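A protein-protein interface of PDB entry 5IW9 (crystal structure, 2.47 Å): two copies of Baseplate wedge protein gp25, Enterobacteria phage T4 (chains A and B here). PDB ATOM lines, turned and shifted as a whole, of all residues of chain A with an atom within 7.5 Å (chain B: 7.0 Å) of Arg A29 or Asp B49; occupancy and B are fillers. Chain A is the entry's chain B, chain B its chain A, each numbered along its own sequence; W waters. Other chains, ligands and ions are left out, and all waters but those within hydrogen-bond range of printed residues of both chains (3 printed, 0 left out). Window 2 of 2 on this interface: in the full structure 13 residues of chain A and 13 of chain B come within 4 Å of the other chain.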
ATOM      1  N   SER A  23      -4.146   8.503  16.123  1.00  0.00           N
ATOM      2  CA  SER A  23      -3.032   9.062  15.354  1.00  0.00           C
ATOM      3  C   SER A  23      -1.746   8.288  15.607  1.00  0.00           C
ATOM      4  O   SER A  23      -0.922   8.120  14.703  1.00  0.00           O
ATOM      5  CB  SER A  23      -2.826  10.539  15.701  1.00  0.00           C
ATOM      6  OG  SER A  23      -3.969  11.312  15.396  1.00  0.00           O
ATOM      7  N   ARG A  24      -1.555   7.825  16.842  1.00  0.00           N
ATOM      8  CA  ARG A  24      -0.389   7.016  17.167  1.00  0.00           C
ATOM      9  C   ARG A  24      -0.431   5.676  16.443  1.00  0.00           C
ATOM     10  O   ARG A  24       0.603   5.187  15.975  1.00  0.00           O
ATOM     11  CB  ARG A  24      -0.309   6.818  18.682  1.00  0.00           C
ATOM     12  CG  ARG A  24       0.544   5.646  19.103  1.00  0.00           C
ATOM     13  CD  ARG A  24       0.473   5.413  20.595  1.00  0.00           C
ATOM     14  NE  ARG A  24       1.077   4.136  20.952  1.00  0.00           N
ATOM     15  CZ  ARG A  24       1.220   3.697  22.196  1.00  0.00           C
ATOM     16  NH1 ARG A  24       1.782   2.517  22.421  1.00  0.00           N
ATOM     17  NH2 ARG A  24       0.807   4.438  23.215  1.00  0.00           N
ATOM     18  N   SER A  25      -1.618   5.073  16.330  1.00  0.00           N
ATOM     19  CA  SER A  25      -1.748   3.824  15.583  1.00  0.00           C
ATOM     20  C   SER A  25      -1.419   4.024  14.107  1.00  0.00           C
ATOM     21  O   SER A  25      -0.701   3.217  13.505  1.00  0.00           O
ATOM     22  CB  SER A  25      -3.158   3.260  15.742  1.00  0.00           C
ATOM     23  OG  SER A  25      -3.263   2.509  16.933  1.00  0.00           O
ATOM     24  N   LEU A  26      -1.958   5.087  13.502  1.00  0.00           N
ATOM     25  CA  LEU A  26      -1.641   5.380  12.107  1.00  0.00           C
ATOM     26  C   LEU A  26      -0.148   5.637  11.929  1.00  0.00           C
ATOM     27  O   LEU A  26       0.460   5.189  10.945  1.00  0.00           O
ATOM     28  CB  LEU A  26      -2.460   6.578  11.627  1.00  0.00           C
ATOM     29  CG  LEU A  26      -3.977   6.380  11.676  1.00  0.00           C
ATOM     30  CD1 LEU A  26      -4.711   7.693  11.450  1.00  0.00           C
ATOM     31  CD2 LEU A  26      -4.411   5.333  10.658  1.00  0.00           C
ATOM     32  N   GLY A  27       0.462   6.344  12.884  1.00  0.00           N
ATOM     33  CA  GLY A  27       1.894   6.576  12.817  1.00  0.00           C
ATOM     34  C   GLY A  27       2.693   5.290  12.910  1.00  0.00           C
ATOM     35  O   GLY A  27       3.697   5.124  12.218  1.00  0.00           O
ATOM     36  N   LEU A  28       2.249   4.359  13.760  1.00  0.00           N
ATOM     37  CA  LEU A  28       2.931   3.075  13.880  1.00  0.00           C
ATOM     38  C   LEU A  28       2.815   2.267  12.595  1.00  0.00           C
ATOM     39  O   LEU A  28       3.792   1.643  12.157  1.00  0.00           O
ATOM     40  CB  LEU A  28       2.366   2.286  15.061  1.00  0.00           C
ATOM     41  CG  LEU A  28       2.974   0.898  15.275  1.00  0.00           C
ATOM     42  CD1 LEU A  28       4.493   0.987  15.414  1.00  0.00           C
ATOM     43  CD2 LEU A  28       2.359   0.219  16.493  1.00  0.00           C
ATOM     44  N   ARG A  29       1.630   2.263  11.977  1.00  0.00           N
ATOM     45  CA  ARG A  29       1.483   1.567  10.703  1.00  0.00           C
ATOM     46  C   ARG A  29       2.405   2.165   9.642  1.00  0.00           C
ATOM     47  O   ARG A  29       3.067   1.430   8.890  1.00  0.00           O
ATOM     48  CB  ARG A  29       0.025   1.611  10.248  1.00  0.00           C
ATOM     49  CG  ARG A  29      -0.236   0.843   8.965  1.00  0.00           C
ATOM     50  CD  ARG A  29      -1.659   1.040   8.478  1.00  0.00           C
ATOM     51  NE  ARG A  29      -1.922   2.435   8.145  1.00  0.00           N
ATOM     52  CZ  ARG A  29      -3.092   2.896   7.714  1.00  0.00           C
ATOM     53  NH1 ARG A  29      -4.118   2.073   7.564  1.00  0.00           N
ATOM     54  NH2 ARG A  29      -3.236   4.183   7.433  1.00  0.00           N
ATOM     55  N   SER A  30       2.484   3.499   9.584  1.00  0.00           N
ATOM     56  CA  SER A  30       3.377   4.121   8.611  1.00  0.00           C
ATOM     57  C   SER A  30       4.840   3.821   8.921  1.00  0.00           C
ATOM     58  O   SER A  30       5.649   3.671   7.996  1.00  0.00           O
ATOM     59  CB  SER A  30       3.128   5.631   8.550  1.00  0.00           C
ATOM     60  OG  SER A  30       3.607   6.287   9.708  1.00  0.00           O
ATOM     61  N   ILE A  31       5.190   3.696  10.204  1.00  0.00           N
ATOM     62  CA  ILE A  31       6.559   3.352  10.578  1.00  0.00           C
ATOM     63  C   ILE A  31       6.900   1.935  10.136  1.00  0.00           C
ATOM     64  O   ILE A  31       7.983   1.689   9.594  1.00  0.00           O
ATOM     65  CB  ILE A  31       6.771   3.532  12.093  1.00  0.00           C
ATOM     66  CG1 ILE A  31       6.841   5.016  12.455  1.00  0.00           C
ATOM     67  CG2 ILE A  31       8.037   2.801  12.554  1.00  0.00           C
ATOM     68  CD1 ILE A  31       6.724   5.279  13.941  1.00  0.00           C
ATOM     69  N   LYS A  32       5.997   0.976  10.372  1.00  0.00           N
ATOM     70  CA  LYS A  32       6.268  -0.393   9.942  1.00  0.00           C
ATOM     71  C   LYS A  32       6.408  -0.475   8.427  1.00  0.00           C
ATOM     72  O   LYS A  32       7.286  -1.182   7.911  1.00  0.00           O
ATOM     73  CB  LYS A  32       5.169  -1.337  10.433  1.00  0.00           C
ATOM     74  CG  LYS A  32       5.119  -1.492  11.946  1.00  0.00           C
ATOM     75  CD  LYS A  32       4.100  -2.545  12.358  1.00  0.00           C
ATOM     76  CE  LYS A  32       4.276  -2.937  13.816  1.00  0.00           C
ATOM     77  NZ  LYS A  32       3.321  -4.007  14.213  1.00  0.00           N
ATOM     78  N   ASN A  33       5.563   0.255   7.694  1.00  0.00           N
ATOM     79  CA  ASN A  33       5.689   0.244   6.240  1.00  0.00           C
ATOM     80  C   ASN A  33       7.014   0.858   5.791  1.00  0.00           C
ATOM     81  O   ASN A  33       7.673   0.339   4.875  1.00  0.00           O
ATOM     82  CB  ASN A  33       4.496   0.960   5.608  1.00  0.00           C
ATOM     83  CG  ASN A  33       3.279   0.062   5.501  1.00  0.00           C
ATOM     84  OD1 ASN A  33       3.256  -0.867   4.696  1.00  0.00           O
ATOM     85  ND2 ASN A  33       2.264   0.330   6.315  1.00  0.00           N
ATOM     86  N   SER A  34       7.432   1.949   6.437  1.00  0.00           N
ATOM     87  CA  SER A  34       8.736   2.539   6.137  1.00  0.00           C
ATOM     88  C   SER A  34       9.868   1.557   6.421  1.00  0.00           C
ATOM     89  O   SER A  34      10.816   1.440   5.632  1.00  0.00           O
ATOM     90  CB  SER A  34       8.916   3.828   6.942  1.00  0.00           C
ATOM     91  OG  SER A  34      10.283   4.164   7.091  1.00  0.00           O
ATOM     92  N   LEU A  35       9.780   0.840   7.547  1.00  0.00           N
ATOM     93  CA  LEU A  35      10.760  -0.189   7.879  1.00  0.00           C
ATOM     94  C   LEU A  35      10.863  -1.228   6.775  1.00  0.00           C
ATOM     95  O   LEU A  35      11.965  -1.576   6.335  1.00  0.00           O
ATOM     96  CB  LEU A  35      10.386  -0.870   9.195  1.00  0.00           C
ATOM     97  CG  LEU A  35      10.945  -0.288  10.487  1.00  0.00           C
ATOM     98  CD1 LEU A  35      10.474  -1.118  11.673  1.00  0.00           C
ATOM     99  CD2 LEU A  35      12.460  -0.250  10.411  1.00  0.00           C
ATOM    100  N   LEU A  36       9.719  -1.757   6.332  1.00  0.00           N
ATOM    101  CA  LEU A  36       9.756  -2.759   5.273  1.00  0.00           C
ATOM    102  C   LEU A  36      10.411  -2.198   4.018  1.00  0.00           C
ATOM    103  O   LEU A  36      11.258  -2.861   3.400  1.00  0.00           O
ATOM    104  CB  LEU A  36       8.344  -3.265   4.968  1.00  0.00           C
ATOM    105  CG  LEU A  36       8.334  -4.534   4.112  1.00  0.00           C
ATOM    106  CD1 LEU A  36       9.150  -5.612   4.801  1.00  0.00           C
ATOM    107  CD2 LEU A  36       6.920  -5.026   3.847  1.00  0.00           C
ATOM    108  N   ARG A  86      12.028   8.115  13.538  1.00  0.00           N
ATOM    109  CA  ARG A  86      10.963   8.003  14.525  1.00  0.00           C
ATOM    110  C   ARG A  86      11.143   6.805  15.449  1.00  0.00           C
ATOM    111  O   ARG A  86      10.412   6.691  16.440  1.00  0.00           O
ATOM    112  CB  ARG A  86       9.598   7.919  13.832  1.00  0.00           C
ATOM    113  CG  ARG A  86       9.176   9.207  13.136  1.00  0.00           C
ATOM    114  CD  ARG A  86       7.964   8.996  12.241  1.00  0.00           C
ATOM    115  NE  ARG A  86       8.283   8.162  11.088  1.00  0.00           N
ATOM    116  CZ  ARG A  86       7.395   7.756  10.187  1.00  0.00           C
ATOM    117  NH1 ARG A  86       6.118   8.102  10.303  1.00  0.00           N
ATOM    118  NH2 ARG A  86       7.785   6.996   9.171  1.00  0.00           N
ATOM    119  N   ARG B  42       3.090  -1.029  -5.427  1.00  0.00           N
ATOM    120  CA  ARG B  42       1.766  -1.296  -5.975  1.00  0.00           C
ATOM    121  C   ARG B  42       0.791  -1.604  -4.845  1.00  0.00           C
ATOM    122  O   ARG B  42       1.033  -2.503  -4.034  1.00  0.00           O
ATOM    123  CB  ARG B  42       1.830  -2.455  -6.966  1.00  0.00           C
ATOM    124  CG  ARG B  42       0.495  -2.819  -7.592  1.00  0.00           C
ATOM    125  CD  ARG B  42       0.693  -3.360  -8.998  1.00  0.00           C
ATOM    126  NE  ARG B  42       1.159  -2.321  -9.913  1.00  0.00           N
ATOM    127  CZ  ARG B  42       1.674  -2.559 -11.115  1.00  0.00           C
ATOM    128  NH1 ARG B  42       2.070  -1.550 -11.880  1.00  0.00           N
ATOM    129  NH2 ARG B  42       1.802  -3.805 -11.548  1.00  0.00           N
ATOM    130  N   LYS B  43      -0.307  -0.853  -4.790  1.00  0.00           N
ATOM    131  CA  LYS B  43      -1.289  -1.044  -3.733  1.00  0.00           C
ATOM    132  C   LYS B  43      -1.875  -2.449  -3.795  1.00  0.00           C
ATOM    133  O   LYS B  43      -2.319  -2.905  -4.853  1.00  0.00           O
ATOM    134  CB  LYS B  43      -2.399   0.001  -3.847  1.00  0.00           C
ATOM    135  CG  LYS B  43      -3.376  -0.020  -2.688  1.00  0.00           C
ATOM    136  CD  LYS B  43      -4.319   1.168  -2.732  1.00  0.00           C
ATOM    137  CE  LYS B  43      -5.245   1.170  -1.530  1.00  0.00           C
ATOM    138  NZ  LYS B  43      -6.092   2.389  -1.490  1.00  0.00           N
ATOM    139  N   GLY B  44      -1.861  -3.139  -2.657  1.00  0.00           N
ATOM    140  CA  GLY B  44      -2.323  -4.507  -2.572  1.00  0.00           C
ATOM    141  C   GLY B  44      -1.234  -5.553  -2.673  1.00  0.00           C
ATOM    142  O   GLY B  44      -1.504  -6.729  -2.401  1.00  0.00           O
ATOM    143  N   SER B  45      -0.014  -5.166  -3.052  1.00  0.00           N
ATOM    144  CA  SER B  45       1.069  -6.129  -3.213  1.00  0.00           C
ATOM    145  C   SER B  45       1.737  -6.489  -1.894  1.00  0.00           C
ATOM    146  O   SER B  45       2.370  -7.546  -1.801  1.00  0.00           O
ATOM    147  CB  SER B  45       2.122  -5.584  -4.179  1.00  0.00           C
ATOM    148  OG  SER B  45       2.784  -4.459  -3.627  1.00  0.00           O
ATOM    149  N   ARG B  46       1.614  -5.637  -0.880  1.00  0.00           N
ATOM    150  CA  ARG B  46       2.247  -5.877   0.406  1.00  0.00           C
ATOM    151  C   ARG B  46       1.267  -6.634   1.293  1.00  0.00           C
ATOM    152  O   ARG B  46       0.249  -6.055   1.703  1.00  0.00           O
ATOM    153  CB  ARG B  46       2.655  -4.558   1.044  1.00  0.00           C
ATOM    154  CG  ARG B  46       3.485  -4.678   2.295  1.00  0.00           C
ATOM    155  CD  ARG B  46       4.039  -3.315   2.700  1.00  0.00           C
ATOM    156  NE  ARG B  46       5.170  -2.900   1.870  1.00  0.00           N
ATOM    157  CZ  ARG B  46       5.891  -1.804   2.088  1.00  0.00           C
ATOM    158  NH1 ARG B  46       5.599  -1.010   3.110  1.00  0.00           N
ATOM    159  NH2 ARG B  46       6.907  -1.499   1.290  1.00  0.00           N
ATOM    160  N   PRO B  47       1.510  -7.912   1.603  1.00  0.00           N
ATOM    161  CA  PRO B  47       0.490  -8.695   2.324  1.00  0.00           C
ATOM    162  C   PRO B  47       0.275  -8.244   3.758  1.00  0.00           C
ATOM    163  O   PRO B  47      -0.829  -8.421   4.289  1.00  0.00           O
ATOM    164  CB  PRO B  47       1.034 -10.132   2.267  1.00  0.00           C
ATOM    165  CG  PRO B  47       2.116 -10.112   1.221  1.00  0.00           C
ATOM    166  CD  PRO B  47       2.678  -8.728   1.234  1.00  0.00           C
ATOM    167  N   PHE B  48       1.294  -7.677   4.406  1.00  0.00           N
ATOM    168  CA  PHE B  48       1.129  -7.175   5.763  1.00  0.00           C
ATOM    169  C   PHE B  48       0.230  -5.949   5.818  1.00  0.00           C
ATOM    170  O   PHE B  48      -0.306  -5.634   6.885  1.00  0.00           O
ATOM    171  CB  PHE B  48       2.493  -6.843   6.364  1.00  0.00           C
ATOM    172  CG  PHE B  48       3.565  -7.818   5.985  1.00  0.00           C
ATOM    173  CD1 PHE B  48       3.481  -9.143   6.380  1.00  0.00           C
ATOM    174  CD2 PHE B  48       4.650  -7.415   5.226  1.00  0.00           C
ATOM    175  CE1 PHE B  48       4.466 -10.047   6.030  1.00  0.00           C
ATOM    176  CE2 PHE B  48       5.638  -8.315   4.873  1.00  0.00           C
ATOM    177  CZ  PHE B  48       5.546  -9.631   5.277  1.00  0.00           C
ATOM    178  N   ASP B  49       0.057  -5.256   4.695  1.00  0.00           N
ATOM    179  CA  ASP B  49      -0.781  -4.059   4.637  1.00  0.00           C
ATOM    180  C   ASP B  49      -1.256  -3.901   3.204  1.00  0.00           C
ATOM    181  O   ASP B  49      -0.631  -3.198   2.396  1.00  0.00           O
ATOM    182  CB  ASP B  49      -0.027  -2.817   5.106  1.00  0.00           C
ATOM    183  CG  ASP B  49      -0.920  -1.592   5.213  1.00  0.00           C
ATOM    184  OD1 ASP B  49      -2.082  -1.637   4.757  1.00  0.00           O
ATOM    185  OD2 ASP B  49      -0.448  -0.569   5.750  1.00  0.00           O
ATOM    186  N   PRO B  50      -2.367  -4.552   2.844  1.00  0.00           N
ATOM    187  CA  PRO B  50      -2.874  -4.450   1.464  1.00  0.00           C
ATOM    188  C   PRO B  50      -3.298  -3.045   1.071  1.00  0.00           C
ATOM    189  O   PRO B  50      -3.521  -2.799  -0.121  1.00  0.00           O
ATOM    190  CB  PRO B  50      -4.073  -5.414   1.454  1.00  0.00           C
ATOM    191  CG  PRO B  50      -3.861  -6.318   2.638  1.00  0.00           C
ATOM    192  CD  PRO B  50      -3.162  -5.483   3.665  1.00  0.00           C
ATOM    193  N   GLU B  51      -3.424  -2.126   2.025  1.00  0.00           N
ATOM    194  CA  GLU B  51      -3.787  -0.747   1.735  1.00  0.00           C
ATOM    195  C   GLU B  51      -2.593   0.120   1.360  1.00  0.00           C
ATOM    196  O   GLU B  51      -2.788   1.222   0.835  1.00  0.00           O
ATOM    197  CB  GLU B  51      -4.496  -0.122   2.943  1.00  0.00           C
ATOM    198  CG  GLU B  51      -5.760  -0.842   3.374  1.00  0.00           C
ATOM    199  CD  GLU B  51      -6.772  -0.952   2.255  1.00  0.00           C
ATOM    200  OE1 GLU B  51      -7.214  -2.084   1.964  1.00  0.00           O
ATOM    201  OE2 GLU B  51      -7.114   0.091   1.660  1.00  0.00           O
ATOM    202  N   PHE B  52      -1.372  -0.342   1.617  1.00  0.00           N
ATOM    203  CA  PHE B  52      -0.188   0.469   1.375  1.00  0.00           C
ATOM    204  C   PHE B  52       0.139   0.527  -0.112  1.00  0.00           C
ATOM    205  O   PHE B  52       0.104  -0.489  -0.813  1.00  0.00           O
ATOM    206  CB  PHE B  52       1.010  -0.087   2.146  1.00  0.00           C
ATOM    207  CG  PHE B  52       2.275   0.700   1.945  1.00  0.00           C
ATOM    208  CD1 PHE B  52       2.529   1.833   2.706  1.00  0.00           C
ATOM    209  CD2 PHE B  52       3.211   0.308   0.999  1.00  0.00           C
ATOM    210  CE1 PHE B  52       3.691   2.561   2.524  1.00  0.00           C
ATOM    211  CE2 PHE B  52       4.374   1.034   0.812  1.00  0.00           C
ATOM    212  CZ  PHE B  52       4.616   2.159   1.577  1.00  0.00           C
ATOM    213  N   GLY B  53       0.458   1.722  -0.586  1.00  0.00           N
ATOM    214  CA  GLY B  53       0.921   1.921  -1.943  1.00  0.00           C
ATOM    215  C   GLY B  53      -0.070   2.709  -2.781  1.00  0.00           C
ATOM    216  O   GLY B  53      -1.064   3.251  -2.289  1.00  0.00           O
ATOM    217  N   ARG B  81      -1.197  11.091   2.521  1.00  0.00           N
ATOM    218  CA  ARG B  81      -1.858  11.467   3.765  1.00  0.00           C
ATOM    219  C   ARG B  81      -2.006  10.273   4.696  1.00  0.00           C
ATOM    220  O   ARG B  81      -1.923  10.424   5.921  1.00  0.00           O
ATOM    221  CB  ARG B  81      -3.227  12.084   3.476  1.00  0.00           C
ATOM    222  CG  ARG B  81      -3.167  13.434   2.786  1.00  0.00           C
ATOM    223  CD  ARG B  81      -2.236  14.384   3.524  1.00  0.00           C
ATOM    224  NE  ARG B  81      -2.435  15.772   3.115  1.00  0.00           N
ATOM    225  CZ  ARG B  81      -1.680  16.786   3.524  1.00  0.00           C
ATOM    226  NH1 ARG B  81      -0.667  16.569   4.353  1.00  0.00           N
ATOM    227  NH2 ARG B  81      -1.937  18.017   3.102  1.00  0.00           N
ATOM    228  N   ASN B  82      -2.205   9.080   4.135  1.00  0.00           N
ATOM    229  CA  ASN B  82      -2.404   7.896   4.958  1.00  0.00           C
ATOM    230  C   ASN B  82      -1.098   7.323   5.499  1.00  0.00           C
ATOM    231  O   ASN B  82      -1.102   6.706   6.571  1.00  0.00           O
ATOM    232  CB  ASN B  82      -3.142   6.822   4.157  1.00  0.00           C
ATOM    233  CG  ASN B  82      -4.632   7.083   4.075  1.00  0.00           C
ATOM    234  OD1 ASN B  82      -5.216   7.684   4.975  1.00  0.00           O
ATOM    235  ND2 ASN B  82      -5.254   6.630   2.995  1.00  0.00           N
ATOM    236  N   TYR B  83       0.025   7.504   4.794  1.00  0.00           N
ATOM    237  CA  TYR B  83       1.230   6.757   5.136  1.00  0.00           C
ATOM    238  C   TYR B  83       2.469   7.621   5.354  1.00  0.00           C
ATOM    239  O   TYR B  83       3.556   7.073   5.574  1.00  0.00           O
ATOM    240  CB  TYR B  83       1.496   5.692   4.066  1.00  0.00           C
ATOM    241  CG  TYR B  83       0.554   4.519   4.197  1.00  0.00           C
ATOM    242  CD1 TYR B  83       0.705   3.608   5.232  1.00  0.00           C
ATOM    243  CD2 TYR B  83      -0.501   4.334   3.308  1.00  0.00           C
ATOM    244  CE1 TYR B  83      -0.152   2.537   5.377  1.00  0.00           C
ATOM    245  CE2 TYR B  83      -1.371   3.254   3.445  1.00  0.00           C
ATOM    246  CZ  TYR B  83      -1.187   2.363   4.484  1.00  0.00           C
ATOM    247  OH  TYR B  83      -2.030   1.287   4.639  1.00  0.00           O
HETATM  248  O   HOH W   1       4.517   4.512   5.605  1.00  0.00           O
HETATM  249  O   HOH W   2      -0.560   4.784   8.339  1.00  0.00           O
HETATM  250  O   HOH W   3       5.972   7.358   7.105  1.00  0.00           O
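The guanidinium group (NH1) of Arg B46 lies within hydrogen-bond range of the side-chain amide oxygen (OD1) of Asn A33 (2.8 Å). The side-chain carboxylate (OD2) of Asp B49 lies within hydrogen-bond range of the side-chain amide nitrogen (ND2) of Asn A33 (2.9 Å). O of Asn B82 lies within hydrogen-bond range of NH2 of Arg A29 (3.4 Å).
OG of Ser A30 lies within hydrogen-bond range of NH1 of Arg A86, 3.2 Å away. N of Phe B52 lies within hydrogen-bond range of OD1 of Asp B49, at 3.5 Å. OD1 of Asp B49 sits close to N of Glu B51 (3.1 Å). The backbone NH (N) of Phe B52 sits at hydrogen-bond distance from the side-chain hydroxyl (OH) of Tyr B83 (3.5 Å). OD2 of Asp B49 is in hydrogen-bond range of OH of Tyr B83, at 2.7 Å. The backbone carbonyl oxygen (O) of Arg A29 sits at hydrogen-bond distance from the side-chain amide nitrogen (ND2) of Asn A33, 2.9 Å away.
Among the printed residues, merely in contact across the chains: Arg A29 with Tyr B83, Asn A33 with Phe B52, Ser A30 with Tyr B83, Leu A36 with Arg B46, Arg A29 with Asp B49, Asn A33 with Tyr B83 and Leu A36 with Phe B48.
Of the printed residues of chain B, Arg A29 touches Asp B49 (3.4 Å), Asn B82 (3.4 Å) and Tyr B83 (3.3 Å). Printed residues of chain B within 4 Å of Asn A33: Arg B46 (2.8 Å), Asp B49 (2.9 Å), Phe B52 (3.3 Å) and Tyr B83 (3.4 Å). Arg A86 touches none of the printed residues of chain B. Of the printed residues of chain A, Arg B46 touches Asn A33 (2.8 Å) and Leu A36 (3.4 Å). Of the printed residues of chain A, Phe B48 touches Leu A36 (3.6 Å). Of the printed residues of chain A, Asn B82 touches Arg A29. Printed residues of chain A within 4 Å of Tyr B83: Arg A29, Ser A30 and Asn A33. The nearest residue of chain B that does not touch Arg A29 is Glu B51 (5.1 Å).
Hydrophobic or aromatic side chains of chain A that line the printed part of chain B: Leu A36. Among the printed residues, 10 pairs touch across the chains.
No position is printed for both chains.
Water W2 lies within hydrogen-bond range of O of Asn B82, NE of Arg A29 and O of Leu A26. Water W1 lies within hydrogen-bond range of the backbone carbonyl oxygen (O) of Tyr B83 (2.7 Å) and the backbone carbonyl oxygen (O) of Ser A30 (2.8 Å). Water W3 lies within hydrogen-bond range of NH2 of Arg A86 (2.8 Å) and O of Tyr B83 (2.9 Å).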
